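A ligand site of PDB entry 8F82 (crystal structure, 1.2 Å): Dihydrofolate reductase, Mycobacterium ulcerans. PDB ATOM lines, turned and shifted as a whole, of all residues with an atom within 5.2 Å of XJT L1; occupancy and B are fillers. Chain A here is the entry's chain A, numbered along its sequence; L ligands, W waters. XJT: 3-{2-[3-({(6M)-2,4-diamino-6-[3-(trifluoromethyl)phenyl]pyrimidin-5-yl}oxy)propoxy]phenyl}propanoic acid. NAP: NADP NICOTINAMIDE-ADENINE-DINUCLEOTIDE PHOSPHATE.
Water W2 bridges O3 of XJT L1 and ND1 of His 64.
Water W1 lies within hydrogen-bond range of the side-chain hydroxyl (OG1) of Thr 127, the backbone carbonyl oxygen (O) of Glu 125, a nitrogen (N1) of XJT L1, a ring nitrogen (NE2) of His 40 and the backbone carbonyl oxygen (O) of Trp 16.
OD2 of Asp 37 sits at hydrogen-bond distance from N4 of XJT L1 (2.6 Å).
An oxygen (O3) of XJT L1 lies within salt-bridge range of the guanidinium group (NH2) of Arg 70 (2.8 Å).
O of Ile 15 is in hydrogen-bond range of N3 of XJT L1 (2.9 Å).
The backbone carbonyl oxygen (O) of Ile 108 is in hydrogen-bond range of a nitrogen (N3) of XJT L1 (3.0 Å).
The side-chain hydroxyl of Tyr 114 is in hydrogen-bond range of a nitrogen (N3) of XJT L1, at 3.4 Å.
The backbone NH (N) of Ala 17 sits at hydrogen-bond distance from an oxygen (O7N) of NAP L2 (2.9 Å).
N7N of NAP L2 sits at hydrogen-bond distance from O of Ala 17 (2.8 Å).
The backbone NH (N) of Thr 56 sits at hydrogen-bond distance from an oxygen (O2A) of NAP L2 (3.0 Å).
The side-chain hydroxyl (OG1) of Thr 56 is in hydrogen-bond range of an oxygen (O2A) of NAP L2, 2.7 Å away.
The side-chain hydroxyl of Thr 127 sits at hydrogen-bond distance from the side-chain carboxylate of Asp 37, at 2.6 Å.
NE of Arg 70 sits at hydrogen-bond distance from O of Pro 68 (2.9 Å).
OG1 of Thr 45 lies within hydrogen-bond range of NH1 of Arg 70 (3.0 Å).
O of Ile 15 is in hydrogen-bond range of OH of Tyr 114 (2.7 Å).
O of Ile 108 lies within hydrogen-bond range of OH of Tyr 114, 3.1 Å away.
O of Trp 16 is in hydrogen-bond range of N of Thr 127.
The side-chain hydroxyl (OH) of Tyr 114 sits close to the backbone NH (N) of Gly 109, at 3.4 Å.
O of Ile 30 is in hydrogen-bond range of NH1 of Arg 33 (2.9 Å).
The indole nitrogen (NE1) of Trp 32 lies close to a fluorine (F2) of XJT L1 (3.0 Å).
O of Leu 34 sits close to F1 of XJT L1 (3.1 Å).
Merely in contact with XJT L1: Lys 42 (3.1 Å), Phe 41 (3.1 Å), Trp 16 (3.3 Å), His 64 (3.4 Å), Leu 38 (3.4 Å), Pro 61 (3.5 Å), Leu 67 (3.5 Å), Leu 60 (3.5 Å), Ile 30 (3.6 Å), Ala 17 (3.7 Å), Thr 127 (3.9 Å) and Pro 68 (3.99 Å).
Within 4 Å of XJT L1: Ile 15, Trp 16, Ala 17, Ile 30, Trp 32, Leu 34, Asp 37, Leu 38, Phe 41, Lys 42, Leu 60, Pro 61, His 64, Leu 67, Pro 68, Arg 70, Ile 108, Tyr 114 and Thr 127.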
ATOM      1  N   ILE A  15     -12.542 -25.861   3.526  1.00  0.00           N
ATOM      2  CA  ILE A  15     -13.454 -25.334   2.507  1.00  0.00           C
ATOM      3  C   ILE A  15     -13.804 -26.490   1.587  1.00  0.00           C
ATOM      4  O   ILE A  15     -12.911 -27.211   1.140  1.00  0.00           O
ATOM      5  CB  ILE A  15     -12.860 -24.117   1.765  1.00  0.00           C
ATOM      6  CG1 ILE A  15     -13.842 -23.547   0.747  1.00  0.00           C
ATOM      7  CG2 ILE A  15     -11.475 -24.414   1.152  1.00  0.00           C
ATOM      8  CD1 ILE A  15     -13.444 -22.165   0.239  1.00  0.00           C
ATOM      9  N   TRP A  16     -15.108 -26.710   1.367  1.00  0.00           N
ATOM     10  CA  TRP A  16     -15.561 -27.792   0.495  1.00  0.00           C
ATOM     11  C   TRP A  16     -16.930 -27.444  -0.085  1.00  0.00           C
ATOM     12  O   TRP A  16     -17.650 -26.593   0.450  1.00  0.00           O
ATOM     13  CB  TRP A  16     -15.627 -29.154   1.193  1.00  0.00           C
ATOM     14  CG  TRP A  16     -16.751 -29.382   2.176  1.00  0.00           C
ATOM     15  CD1 TRP A  16     -18.014 -29.848   1.892  1.00  0.00           C
ATOM     16  CD2 TRP A  16     -16.691 -29.252   3.602  1.00  0.00           C
ATOM     17  NE1 TRP A  16     -18.740 -29.991   3.048  1.00  0.00           N
ATOM     18  CE2 TRP A  16     -17.950 -29.630   4.113  1.00  0.00           C
ATOM     19  CE3 TRP A  16     -15.699 -28.833   4.499  1.00  0.00           C
ATOM     20  CZ2 TRP A  16     -18.232 -29.620   5.470  1.00  0.00           C
ATOM     21  CZ3 TRP A  16     -15.988 -28.810   5.853  1.00  0.00           C
ATOM     22  CH2 TRP A  16     -17.250 -29.196   6.323  1.00  0.00           C
ATOM     23  N   ALA A  17     -17.269 -28.127  -1.179  1.00  0.00           N
ATOM     24  CA  ALA A  17     -18.601 -28.093  -1.775  1.00  0.00           C
ATOM     25  C   ALA A  17     -19.171 -29.504  -1.767  1.00  0.00           C
ATOM     26  O   ALA A  17     -18.501 -30.438  -2.195  1.00  0.00           O
ATOM     27  CB  ALA A  17     -18.531 -27.557  -3.209  1.00  0.00           C
ATOM     28  N   ILE A  30     -15.381 -34.306  -9.370  1.00  0.00           N
ATOM     29  CA  ILE A  30     -16.522 -33.811  -8.630  1.00  0.00           C
ATOM     30  C   ILE A  30     -17.756 -33.993  -9.505  1.00  0.00           C
ATOM     31  O   ILE A  30     -17.773 -33.550 -10.656  1.00  0.00           O
ATOM     32  CB  ILE A  30     -16.334 -32.329  -8.252  1.00  0.00           C
ATOM     33  CG1 ILE A  30     -15.047 -32.182  -7.420  1.00  0.00           C
ATOM     34  CG2 ILE A  30     -17.558 -31.797  -7.504  1.00  0.00           C
ATOM     35  CD1 ILE A  30     -14.660 -30.740  -7.106  1.00  0.00           C
ATOM     36  N   TRP A  32     -20.600 -32.853 -10.386  1.00  0.00           N
ATOM     37  CA  TRP A  32     -21.472 -31.801 -10.895  1.00  0.00           C
ATOM     38  C   TRP A  32     -20.557 -30.655 -11.308  1.00  0.00           C
ATOM     39  O   TRP A  32     -19.351 -30.676 -11.053  1.00  0.00           O
ATOM     40  CB  TRP A  32     -22.511 -31.327  -9.848  1.00  0.00           C
ATOM     41  CG  TRP A  32     -21.876 -30.646  -8.677  1.00  0.00           C
ATOM     42  CD1 TRP A  32     -21.529 -29.331  -8.585  1.00  0.00           C
ATOM     43  CD2 TRP A  32     -21.441 -31.250  -7.452  1.00  0.00           C
ATOM     44  NE1 TRP A  32     -20.907 -29.089  -7.387  1.00  0.00           N
ATOM     45  CE2 TRP A  32     -20.838 -30.256  -6.677  1.00  0.00           C
ATOM     46  CE3 TRP A  32     -21.504 -32.560  -6.956  1.00  0.00           C
ATOM     47  CZ2 TRP A  32     -20.303 -30.502  -5.405  1.00  0.00           C
ATOM     48  CZ3 TRP A  32     -20.973 -32.809  -5.693  1.00  0.00           C
ATOM     49  CH2 TRP A  32     -20.384 -31.784  -4.934  1.00  0.00           C
ATOM     50  N   ARG A  33     -21.123 -29.656 -11.965  1.00  0.00           N
ATOM     51  CA  ARG A  33     -20.398 -28.452 -12.345  1.00  0.00           C
ATOM     52  C   ARG A  33     -21.061 -27.261 -11.683  1.00  0.00           C
ATOM     53  O   ARG A  33     -22.300 -27.160 -11.670  1.00  0.00           O
ATOM     54  CB  ARG A  33     -20.381 -28.273 -13.869  1.00  0.00           C
ATOM     55  CG  ARG A  33     -19.622 -29.361 -14.618  1.00  0.00           C
ATOM     56  CD  ARG A  33     -18.159 -29.379 -14.228  1.00  0.00           C
ATOM     57  NE  ARG A  33     -17.414 -30.459 -14.872  1.00  0.00           N
ATOM     58  CZ  ARG A  33     -17.109 -31.617 -14.293  1.00  0.00           C
ATOM     59  NH1 ARG A  33     -17.495 -31.899 -13.062  1.00  0.00           N
ATOM     60  NH2 ARG A  33     -16.400 -32.512 -14.978  1.00  0.00           N
ATOM     61  N   LEU A  34     -20.270 -26.345 -11.135  1.00  0.00           N
ATOM     62  CA  LEU A  34     -20.806 -25.167 -10.473  1.00  0.00           C
ATOM     63  C   LEU A  34     -19.798 -24.033 -10.544  1.00  0.00           C
ATOM     64  O   LEU A  34     -19.039 -23.787  -9.595  1.00  0.00           O
ATOM     65  CB  LEU A  34     -21.204 -25.474  -9.036  1.00  0.00           C
ATOM     66  CG  LEU A  34     -21.974 -24.377  -8.297  1.00  0.00           C
ATOM     67  CD1 LEU A  34     -23.188 -23.965  -9.109  1.00  0.00           C
ATOM     68  CD2 LEU A  34     -22.373 -24.889  -6.933  1.00  0.00           C
ATOM     69  N   PRO A  35     -19.777 -23.298 -11.657  1.00  0.00           N
ATOM     70  CA  PRO A  35     -18.767 -22.235 -11.827  1.00  0.00           C
ATOM     71  C   PRO A  35     -18.771 -21.206 -10.710  1.00  0.00           C
ATOM     72  O   PRO A  35     -17.708 -20.696 -10.328  1.00  0.00           O
ATOM     73  CB  PRO A  35     -19.166 -21.603 -13.167  1.00  0.00           C
ATOM     74  CG  PRO A  35     -19.794 -22.723 -13.933  1.00  0.00           C
ATOM     75  CD  PRO A  35     -20.543 -23.543 -12.898  1.00  0.00           C
ATOM     76  N   ASP A  37     -19.318 -21.726  -7.560  1.00  0.00           N
ATOM     77  CA  ASP A  37     -18.567 -22.239  -6.414  1.00  0.00           C
ATOM     78  C   ASP A  37     -17.073 -22.258  -6.683  1.00  0.00           C
ATOM     79  O   ASP A  37     -16.276 -21.928  -5.802  1.00  0.00           O
ATOM     80  CB  ASP A  37     -19.043 -23.608  -5.971  1.00  0.00           C
ATOM     81  CG  ASP A  37     -18.122 -24.201  -4.943  1.00  0.00           C
ATOM     82  OD1 ASP A  37     -18.177 -23.781  -3.767  1.00  0.00           O
ATOM     83  OD2 ASP A  37     -17.296 -25.046  -5.330  1.00  0.00           O
ATOM     84  N   LEU A  38     -16.654 -22.626  -7.897  1.00  0.00           N
ATOM     85  CA  LEU A  38     -15.229 -22.542  -8.209  1.00  0.00           C
ATOM     86  C   LEU A  38     -14.726 -21.115  -8.026  1.00  0.00           C
ATOM     87  O   LEU A  38     -13.641 -20.889  -7.460  1.00  0.00           O
ATOM     88  CB  LEU A  38     -14.974 -23.046  -9.637  1.00  0.00           C
ATOM     89  CG  LEU A  38     -13.558 -22.809 -10.137  1.00  0.00           C
ATOM     90  CD1 LEU A  38     -12.560 -23.393  -9.166  1.00  0.00           C
ATOM     91  CD2 LEU A  38     -13.393 -23.403 -11.520  1.00  0.00           C
ATOM     92  N   HIS A  40     -16.027 -18.830  -5.972  1.00  0.00           N
ATOM     93  CA  HIS A  40     -16.007 -18.621  -4.524  1.00  0.00           C
ATOM     94  C   HIS A  40     -14.739 -19.218  -3.904  1.00  0.00           C
ATOM     95  O   HIS A  40     -14.058 -18.574  -3.102  1.00  0.00           O
ATOM     96  CB  HIS A  40     -17.286 -19.277  -3.961  1.00  0.00           C
ATOM     97  CG  HIS A  40     -17.307 -19.496  -2.479  1.00  0.00           C
ATOM     98  ND1 HIS A  40     -17.551 -18.491  -1.575  1.00  0.00           N
ATOM     99  CD2 HIS A  40     -17.201 -20.635  -1.759  1.00  0.00           C
ATOM    100  CE1 HIS A  40     -17.573 -18.992  -0.353  1.00  0.00           C
ATOM    101  NE2 HIS A  40     -17.361 -20.297  -0.433  1.00  0.00           N
ATOM    102  N   PHE A  41     -14.391 -20.443  -4.316  1.00  0.00           N
ATOM    103  CA  PHE A  41     -13.185 -21.099  -3.810  1.00  0.00           C
ATOM    104  C   PHE A  41     -11.939 -20.300  -4.161  1.00  0.00           C
ATOM    105  O   PHE A  41     -11.065 -20.088  -3.314  1.00  0.00           O
ATOM    106  CB  PHE A  41     -13.113 -22.521  -4.393  1.00  0.00           C
ATOM    107  CG  PHE A  41     -11.821 -23.211  -4.102  1.00  0.00           C
ATOM    108  CD1 PHE A  41     -11.568 -23.738  -2.844  1.00  0.00           C
ATOM    109  CD2 PHE A  41     -10.831 -23.296  -5.077  1.00  0.00           C
ATOM    110  CE1 PHE A  41     -10.363 -24.363  -2.564  1.00  0.00           C
ATOM    111  CE2 PHE A  41      -9.624 -23.912  -4.801  1.00  0.00           C
ATOM    112  CZ  PHE A  41      -9.395 -24.420  -3.540  1.00  0.00           C
ATOM    113  N   LYS A  42     -11.835 -19.855  -5.406  1.00  0.00           N
ATOM    114  CA  LYS A  42     -10.687 -19.044  -5.814  1.00  0.00           C
ATOM    115  C   LYS A  42     -10.624 -17.739  -5.038  1.00  0.00           C
ATOM    116  O   LYS A  42      -9.522 -17.303  -4.645  1.00  0.00           O
ATOM    117  CB  LYS A  42     -10.764 -18.775  -7.321  1.00  0.00           C
ATOM    118  CG  LYS A  42     -10.381 -19.978  -8.152  1.00  0.00           C
ATOM    119  CD  LYS A  42     -10.908 -19.915  -9.588  1.00  0.00           C
ATOM    120  CE  LYS A  42     -10.062 -19.016 -10.496  1.00  0.00           C
ATOM    121  NZ  LYS A  42     -10.602 -19.035 -11.898  1.00  0.00           N
ATOM    122  N   THR A  45      -9.438 -18.445  -1.306  1.00  0.00           N
ATOM    123  CA  THR A  45      -8.122 -19.040  -1.115  1.00  0.00           C
ATOM    124  C   THR A  45      -6.975 -18.243  -1.721  1.00  0.00           C
ATOM    125  O   THR A  45      -5.831 -18.461  -1.314  1.00  0.00           O
ATOM    126  CB  THR A  45      -8.073 -20.500  -1.596  1.00  0.00           C
ATOM    127  OG1 THR A  45      -8.339 -20.576  -3.006  1.00  0.00           O
ATOM    128  CG2 THR A  45      -9.041 -21.384  -0.803  1.00  0.00           C
ATOM    129  N   THR A  56      -6.459 -35.480  -4.094  1.00  0.00           N
ATOM    130  CA  THR A  56      -6.963 -34.206  -4.591  1.00  0.00           C
ATOM    131  C   THR A  56      -5.941 -33.547  -5.517  1.00  0.00           C
ATOM    132  O   THR A  56      -6.308 -33.018  -6.571  1.00  0.00           O
ATOM    133  CB  THR A  56      -7.373 -33.314  -3.421  1.00  0.00           C
ATOM    134  OG1 THR A  56      -8.517 -33.896  -2.792  1.00  0.00           O
ATOM    135  CG2 THR A  56      -7.740 -31.913  -3.882  1.00  0.00           C
ATOM    136  N   SER A  59      -6.279 -34.947  -8.838  1.00  0.00           N
ATOM    137  CA  SER A  59      -7.527 -34.579  -9.496  1.00  0.00           C
ATOM    138  C   SER A  59      -7.484 -33.208 -10.166  1.00  0.00           C
ATOM    139  O   SER A  59      -8.401 -32.889 -10.927  1.00  0.00           O
ATOM    140  CB  SER A  59      -8.684 -34.602  -8.485  1.00  0.00           C
ATOM    141  OG  SER A  59      -8.697 -33.436  -7.662  1.00  0.00           O
ATOM    142  N   LEU A  60      -6.496 -32.380  -9.881  1.00  0.00           N
ATOM    143  CA  LEU A  60      -6.506 -31.015 -10.402  1.00  0.00           C
ATOM    144  C   LEU A  60      -6.176 -31.012 -11.895  1.00  0.00           C
ATOM    145  O   LEU A  60      -5.121 -31.501 -12.286  1.00  0.00           O
ATOM    146  CB  LEU A  60      -5.474 -30.169  -9.664  1.00  0.00           C
ATOM    147  CG  LEU A  60      -5.708 -29.960  -8.171  1.00  0.00           C
ATOM    148  CD1 LEU A  60      -4.521 -29.221  -7.570  1.00  0.00           C
ATOM    149  CD2 LEU A  60      -7.006 -29.210  -7.926  1.00  0.00           C
ATOM    150  N   PRO A  61      -7.021 -30.425 -12.747  1.00  0.00           N
ATOM    151  CA  PRO A  61      -6.691 -30.380 -14.176  1.00  0.00           C
ATOM    152  C   PRO A  61      -5.408 -29.604 -14.432  1.00  0.00           C
ATOM    153  O   PRO A  61      -5.017 -28.736 -13.640  1.00  0.00           O
ATOM    154  CB  PRO A  61      -7.907 -29.674 -14.799  1.00  0.00           C
ATOM    155  CG  PRO A  61      -9.024 -29.976 -13.849  1.00  0.00           C
ATOM    156  CD  PRO A  61      -8.384 -29.940 -12.472  1.00  0.00           C
ATOM    157  N   HIS A  64      -4.857 -26.072 -13.743  1.00  0.00           N
ATOM    158  CA  HIS A  64      -5.056 -25.705 -12.356  1.00  0.00           C
ATOM    159  C   HIS A  64      -4.092 -26.434 -11.421  1.00  0.00           C
ATOM    160  O   HIS A  64      -4.335 -26.514 -10.207  1.00  0.00           O
ATOM    161  CB  HIS A  64      -6.510 -26.002 -11.956  1.00  0.00           C
ATOM    162  CG  HIS A  64      -7.541 -25.339 -12.829  1.00  0.00           C
ATOM    163  ND1 HIS A  64      -7.879 -24.008 -12.720  1.00  0.00           N
ATOM    164  CD2 HIS A  64      -8.315 -25.844 -13.826  1.00  0.00           C
ATOM    165  CE1 HIS A  64      -8.810 -23.724 -13.610  1.00  0.00           C
ATOM    166  NE2 HIS A  64      -9.096 -24.811 -14.296  1.00  0.00           N
ATOM    167  N   LEU A  67      -2.331 -24.948  -8.117  1.00  0.00           N
ATOM    168  CA  LEU A  67      -3.329 -23.880  -8.060  1.00  0.00           C
ATOM    169  C   LEU A  67      -2.606 -22.545  -8.090  1.00  0.00           C
ATOM    170  O   LEU A  67      -1.772 -22.279  -7.223  1.00  0.00           O
ATOM    171  CB  LEU A  67      -4.139 -24.017  -6.770  1.00  0.00           C
ATOM    172  CG  LEU A  67      -5.004 -25.284  -6.753  1.00  0.00           C
ATOM    173  CD1 LEU A  67      -5.504 -25.583  -5.335  1.00  0.00           C
ATOM    174  CD2 LEU A  67      -6.161 -25.181  -7.727  1.00  0.00           C
ATOM    175  N   PRO A  68      -2.895 -21.679  -9.059  1.00  0.00           N
ATOM    176  CA  PRO A  68      -2.101 -20.452  -9.203  1.00  0.00           C
ATOM    177  C   PRO A  68      -2.337 -19.470  -8.055  1.00  0.00           C
ATOM    178  O   PRO A  68      -3.451 -19.343  -7.546  1.00  0.00           O
ATOM    179  CB  PRO A  68      -2.591 -19.860 -10.537  1.00  0.00           C
ATOM    180  CG  PRO A  68      -3.997 -20.450 -10.708  1.00  0.00           C
ATOM    181  CD  PRO A  68      -3.862 -21.856 -10.154  1.00  0.00           C
ATOM    182  N   ARG A  70      -1.279 -19.412  -4.980  1.00  0.00           N
ATOM    183  CA  ARG A  70      -1.439 -19.996  -3.651  1.00  0.00           C
ATOM    184  C   ARG A  70      -0.262 -20.922  -3.398  1.00  0.00           C
ATOM    185  O   ARG A  70       0.283 -21.513  -4.332  1.00  0.00           O
ATOM    186  CB  ARG A  70      -2.737 -20.800  -3.584  1.00  0.00           C
ATOM    187  CG  ARG A  70      -3.944 -19.875  -3.471  1.00  0.00           C
ATOM    188  CD  ARG A  70      -5.217 -20.455  -4.051  1.00  0.00           C
ATOM    189  NE  ARG A  70      -5.207 -20.415  -5.510  1.00  0.00           N
ATOM    190  CZ  ARG A  70      -6.197 -20.862  -6.272  1.00  0.00           C
ATOM    191  NH1 ARG A  70      -7.300 -21.357  -5.747  1.00  0.00           N
ATOM    192  NH2 ARG A  70      -6.066 -20.802  -7.593  1.00  0.00           N
ATOM    193  N   ILE A 108      -8.221 -27.953   1.611  1.00  0.00           N
ATOM    194  CA  ILE A 108      -9.064 -27.899   0.428  1.00  0.00           C
ATOM    195  C   ILE A 108      -9.501 -29.277  -0.048  1.00  0.00           C
ATOM    196  O   ILE A 108     -10.080 -29.400  -1.135  1.00  0.00           O
ATOM    197  CB  ILE A 108      -8.408 -27.086  -0.703  1.00  0.00           C
ATOM    198  CG1 ILE A 108      -7.194 -27.827  -1.293  1.00  0.00           C
ATOM    199  CG2 ILE A 108      -8.022 -25.707  -0.207  1.00  0.00           C
ATOM    200  CD1 ILE A 108      -6.805 -27.325  -2.637  1.00  0.00           C
ATOM    201  N   GLY A 109      -9.253 -30.311   0.759  1.00  0.00           N
ATOM    202  CA  GLY A 109      -9.735 -31.658   0.494  1.00  0.00           C
ATOM    203  C   GLY A 109      -8.596 -32.657   0.401  1.00  0.00           C
ATOM    204  O   GLY A 109      -7.424 -32.293   0.486  1.00  0.00           O
ATOM    205  N   TYR A 114      -9.888 -33.965   5.117  1.00  0.00           N
ATOM    206  CA  TYR A 114     -10.858 -33.223   5.927  1.00  0.00           C
ATOM    207  C   TYR A 114     -11.065 -33.885   7.280  1.00  0.00           C
ATOM    208  O   TYR A 114     -11.175 -33.202   8.303  1.00  0.00           O
ATOM    209  CB  TYR A 114     -12.235 -33.106   5.240  1.00  0.00           C
ATOM    210  CG  TYR A 114     -12.314 -32.196   4.026  1.00  0.00           C
ATOM    211  CD1 TYR A 114     -11.742 -30.922   4.021  1.00  0.00           C
ATOM    212  CD2 TYR A 114     -12.988 -32.617   2.902  1.00  0.00           C
ATOM    213  CE1 TYR A 114     -11.830 -30.118   2.892  1.00  0.00           C
ATOM    214  CE2 TYR A 114     -13.088 -31.818   1.780  1.00  0.00           C
ATOM    215  CZ  TYR A 114     -12.514 -30.574   1.785  1.00  0.00           C
ATOM    216  OH  TYR A 114     -12.604 -29.821   0.642  1.00  0.00           O
ATOM    217  N   GLU A 125     -15.913 -23.360   5.540  1.00  0.00           N
ATOM    218  CA  GLU A 125     -16.700 -22.662   4.524  1.00  0.00           C
ATOM    219  C   GLU A 125     -17.257 -23.719   3.594  1.00  0.00           C
ATOM    220  O   GLU A 125     -16.509 -24.374   2.863  1.00  0.00           O
ATOM    221  CB  GLU A 125     -15.835 -21.655   3.784  1.00  0.00           C
ATOM    222  CG  GLU A 125     -15.393 -20.482   4.650  1.00  0.00           C
ATOM    223  CD  GLU A 125     -16.553 -19.610   5.114  1.00  0.00           C
ATOM    224  OE1 GLU A 125     -17.591 -19.524   4.417  1.00  0.00           O
ATOM    225  OE2 GLU A 125     -16.427 -19.010   6.198  1.00  0.00           O
ATOM    226  N   THR A 127     -20.085 -25.041   0.711  1.00  0.00           N
ATOM    227  CA  THR A 127     -21.100 -24.811  -0.297  1.00  0.00           C
ATOM    228  C   THR A 127     -21.998 -26.034  -0.351  1.00  0.00           C
ATOM    229  O   THR A 127     -21.514 -27.151  -0.526  1.00  0.00           O
ATOM    230  CB  THR A 127     -20.474 -24.559  -1.668  1.00  0.00           C
ATOM    231  OG1 THR A 127     -19.562 -23.449  -1.556  1.00  0.00           O
ATOM    232  CG2 THR A 127     -21.544 -24.224  -2.703  1.00  0.00           C
HETATM  233  N1  XJT L   1     -15.987 -24.761  -2.230  1.00  0.00           N
HETATM  234  C2  XJT L   1     -13.154 -26.812  -2.492  1.00  0.00           C
HETATM  235  C3  XJT L   1     -13.162 -27.143  -3.878  1.00  0.00           C
HETATM  236  C4  XJT L   1     -10.842 -27.437  -4.512  1.00  0.00           C
HETATM  237  C6  XJT L   1     -10.347 -28.802  -6.611  1.00  0.00           C
HETATM  238  C7  XJT L   1     -10.339 -27.619  -8.696  1.00  0.00           C
HETATM  239  C8  XJT L   1     -10.809 -28.743  -9.353  1.00  0.00           C
HETATM  240  C9  XJT L   1     -11.083 -28.678 -10.708  1.00  0.00           C
HETATM  241  C10 XJT L   1     -10.892 -27.506 -11.399  1.00  0.00           C
HETATM  242  C11 XJT L   1     -10.439 -26.381 -10.725  1.00  0.00           C
HETATM  243  C12 XJT L   1     -10.149 -26.404  -9.368  1.00  0.00           C
HETATM  244  C13 XJT L   1      -9.656 -25.166  -8.625  1.00  0.00           C
HETATM  245  C15 XJT L   1      -8.541 -22.887  -8.765  1.00  0.00           C
HETATM  246  C19 XJT L   1     -15.964 -27.331  -7.872  1.00  0.00           C
HETATM  247  C20 XJT L   1     -17.369 -27.645  -8.256  1.00  0.00           C
HETATM  248  C23 XJT L   1     -13.395 -26.722  -7.069  1.00  0.00           C
HETATM  249  C1  XJT L   1     -15.042 -25.554  -2.751  1.00  0.00           C
HETATM  250  C14 XJT L   1      -9.014 -24.123  -9.516  1.00  0.00           C
HETATM  251  C16 XJT L   1     -14.201 -26.630  -4.638  1.00  0.00           C
HETATM  252  C17 XJT L   1     -14.387 -26.858  -6.104  1.00  0.00           C
HETATM  253  C18 XJT L   1     -15.664 -27.126  -6.533  1.00  0.00           C
HETATM  254  C21 XJT L   1     -14.968 -27.191  -8.828  1.00  0.00           C
HETATM  255  C22 XJT L   1     -13.672 -26.892  -8.418  1.00  0.00           C
HETATM  256  C5  XJT L   1     -10.004 -28.502  -5.165  1.00  0.00           C
HETATM  257  F1  XJT L   1     -18.008 -26.596  -8.755  1.00  0.00           F
HETATM  258  F2  XJT L   1     -18.119 -28.064  -7.241  1.00  0.00           F
HETATM  259  F3  XJT L   1     -17.473 -28.596  -9.177  1.00  0.00           F
HETATM  260  N2  XJT L   1     -14.085 -26.031  -1.938  1.00  0.00           N
HETATM  261  N3  XJT L   1     -12.198 -27.327  -1.665  1.00  0.00           N
HETATM  262  N4  XJT L   1     -15.125 -25.842  -4.067  1.00  0.00           N
HETATM  263  O1  XJT L   1     -12.195 -27.939  -4.441  1.00  0.00           O
HETATM  264  O2  XJT L   1     -10.052 -27.608  -7.362  1.00  0.00           O
HETATM  265  O3  XJT L   1      -7.764 -22.114  -9.352  1.00  0.00           O
HETATM  266  O4  XJT L   1      -8.949 -22.681  -7.599  1.00  0.00           O
HETATM  267  PA  NAP L   2      -7.559 -37.059  -0.422  1.00  0.00           P
HETATM  268  O1A NAP L   2      -8.027 -36.850   0.981  1.00  0.00           O
HETATM  269  O2A NAP L   2      -7.457 -35.875  -1.309  1.00  0.00           O
HETATM  270  O5B NAP L   2      -6.134 -37.765  -0.450  1.00  0.00           O
HETATM  271  C5B NAP L   2      -5.901 -39.016   0.203  1.00  0.00           C
HETATM  272  C4B NAP L   2      -4.411 -39.248   0.251  1.00  0.00           C
HETATM  273  O4B NAP L   2      -3.824 -38.389   1.262  1.00  0.00           O
HETATM  274  C3B NAP L   2      -3.973 -40.652   0.650  1.00  0.00           C
HETATM  275  O3B NAP L   2      -4.121 -41.562  -0.427  1.00  0.00           O
HETATM  276  C2B NAP L   2      -2.543 -40.379   1.108  1.00  0.00           C
HETATM  277  O2B NAP L   2      -1.678 -40.145   0.010  1.00  0.00           O
HETATM  278  C1B NAP L   2      -2.722 -39.048   1.845  1.00  0.00           C
HETATM  279  N9A NAP L   2      -2.933 -39.208   3.269  1.00  0.00           N
HETATM  280  C8A NAP L   2      -4.092 -39.525   3.945  1.00  0.00           C
HETATM  281  N7A NAP L   2      -3.924 -39.623   5.241  1.00  0.00           N
HETATM  282  C5A NAP L   2      -2.575 -39.359   5.438  1.00  0.00           C
HETATM  283  C6A NAP L   2      -1.765 -39.312   6.598  1.00  0.00           C
HETATM  284  N6A NAP L   2      -2.222 -39.527   7.832  1.00  0.00           N
HETATM  285  N1A NAP L   2      -0.452 -39.042   6.422  1.00  0.00           N
HETATM  286  C2A NAP L   2       0.008 -38.818   5.183  1.00  0.00           C
HETATM  287  N3A NAP L   2      -0.655 -38.833   4.033  1.00  0.00           N
HETATM  288  C4A NAP L   2      -1.956 -39.118   4.233  1.00  0.00           C
HETATM  289  O3  NAP L   2      -8.442 -38.199  -1.114  1.00  0.00           O
HETATM  290  PN  NAP L   2     -10.019 -38.494  -1.244  1.00  0.00           P
HETATM  291  O1N NAP L   2     -10.643 -38.562   0.106  1.00  0.00           O
HETATM  292  O2N NAP L   2     -10.134 -39.682  -2.143  1.00  0.00           O
HETATM  293  O5D NAP L   2     -10.564 -37.178  -1.967  1.00  0.00           O
HETATM  294  C5D NAP L   2     -10.360 -36.956  -3.386  1.00  0.00           C
HETATM  295  C4D NAP L   2     -11.711 -36.764  -4.043  1.00  0.00           C
HETATM  296  O4D NAP L   2     -12.385 -35.618  -3.484  1.00  0.00           O
HETATM  297  C3D NAP L   2     -11.679 -36.519  -5.562  1.00  0.00           C
HETATM  298  O3D NAP L   2     -12.873 -37.053  -6.121  1.00  0.00           O
HETATM  299  C2D NAP L   2     -11.720 -34.985  -5.644  1.00  0.00           C
HETATM  300  O2D NAP L   2     -12.212 -34.535  -6.893  1.00  0.00           O
HETATM  301  C1D NAP L   2     -12.729 -34.703  -4.528  1.00  0.00           C
HETATM  302  N1N NAP L   2     -12.675 -33.366  -3.930  1.00  0.00           N
HETATM  303  C2N NAP L   2     -13.838 -32.643  -3.808  1.00  0.00           C
HETATM  304  C3N NAP L   2     -13.829 -31.399  -3.193  1.00  0.00           C
HETATM  305  C7N NAP L   2     -15.100 -30.613  -3.074  1.00  0.00           C
HETATM  306  O7N NAP L   2     -15.113 -29.574  -2.399  1.00  0.00           O
HETATM  307  N7N NAP L   2     -16.181 -31.071  -3.694  1.00  0.00           N
HETATM  308  C4N NAP L   2     -12.627 -30.880  -2.711  1.00  0.00           C
HETATM  309  C5N NAP L   2     -11.463 -31.627  -2.836  1.00  0.00           C
HETATM  310  C6N NAP L   2     -11.495 -32.863  -3.423  1.00  0.00           C
HETATM  311  P2B NAP L   2      -0.749 -41.355  -0.535  1.00  0.00           P
HETATM  312  O1X NAP L   2       0.033 -40.681  -1.644  1.00  0.00           O
HETATM  313  O2X NAP L   2       0.115 -41.813   0.625  1.00  0.00           O
HETATM  314  O3X NAP L   2      -1.699 -42.414  -1.048  1.00  0.00           O
HETATM  315  O   HOH W   1     -17.244 -23.318   0.143  1.00  0.00           O
HETATM  316  O   HOH W   2      -7.013 -21.950 -11.660  1.00  0.00           O
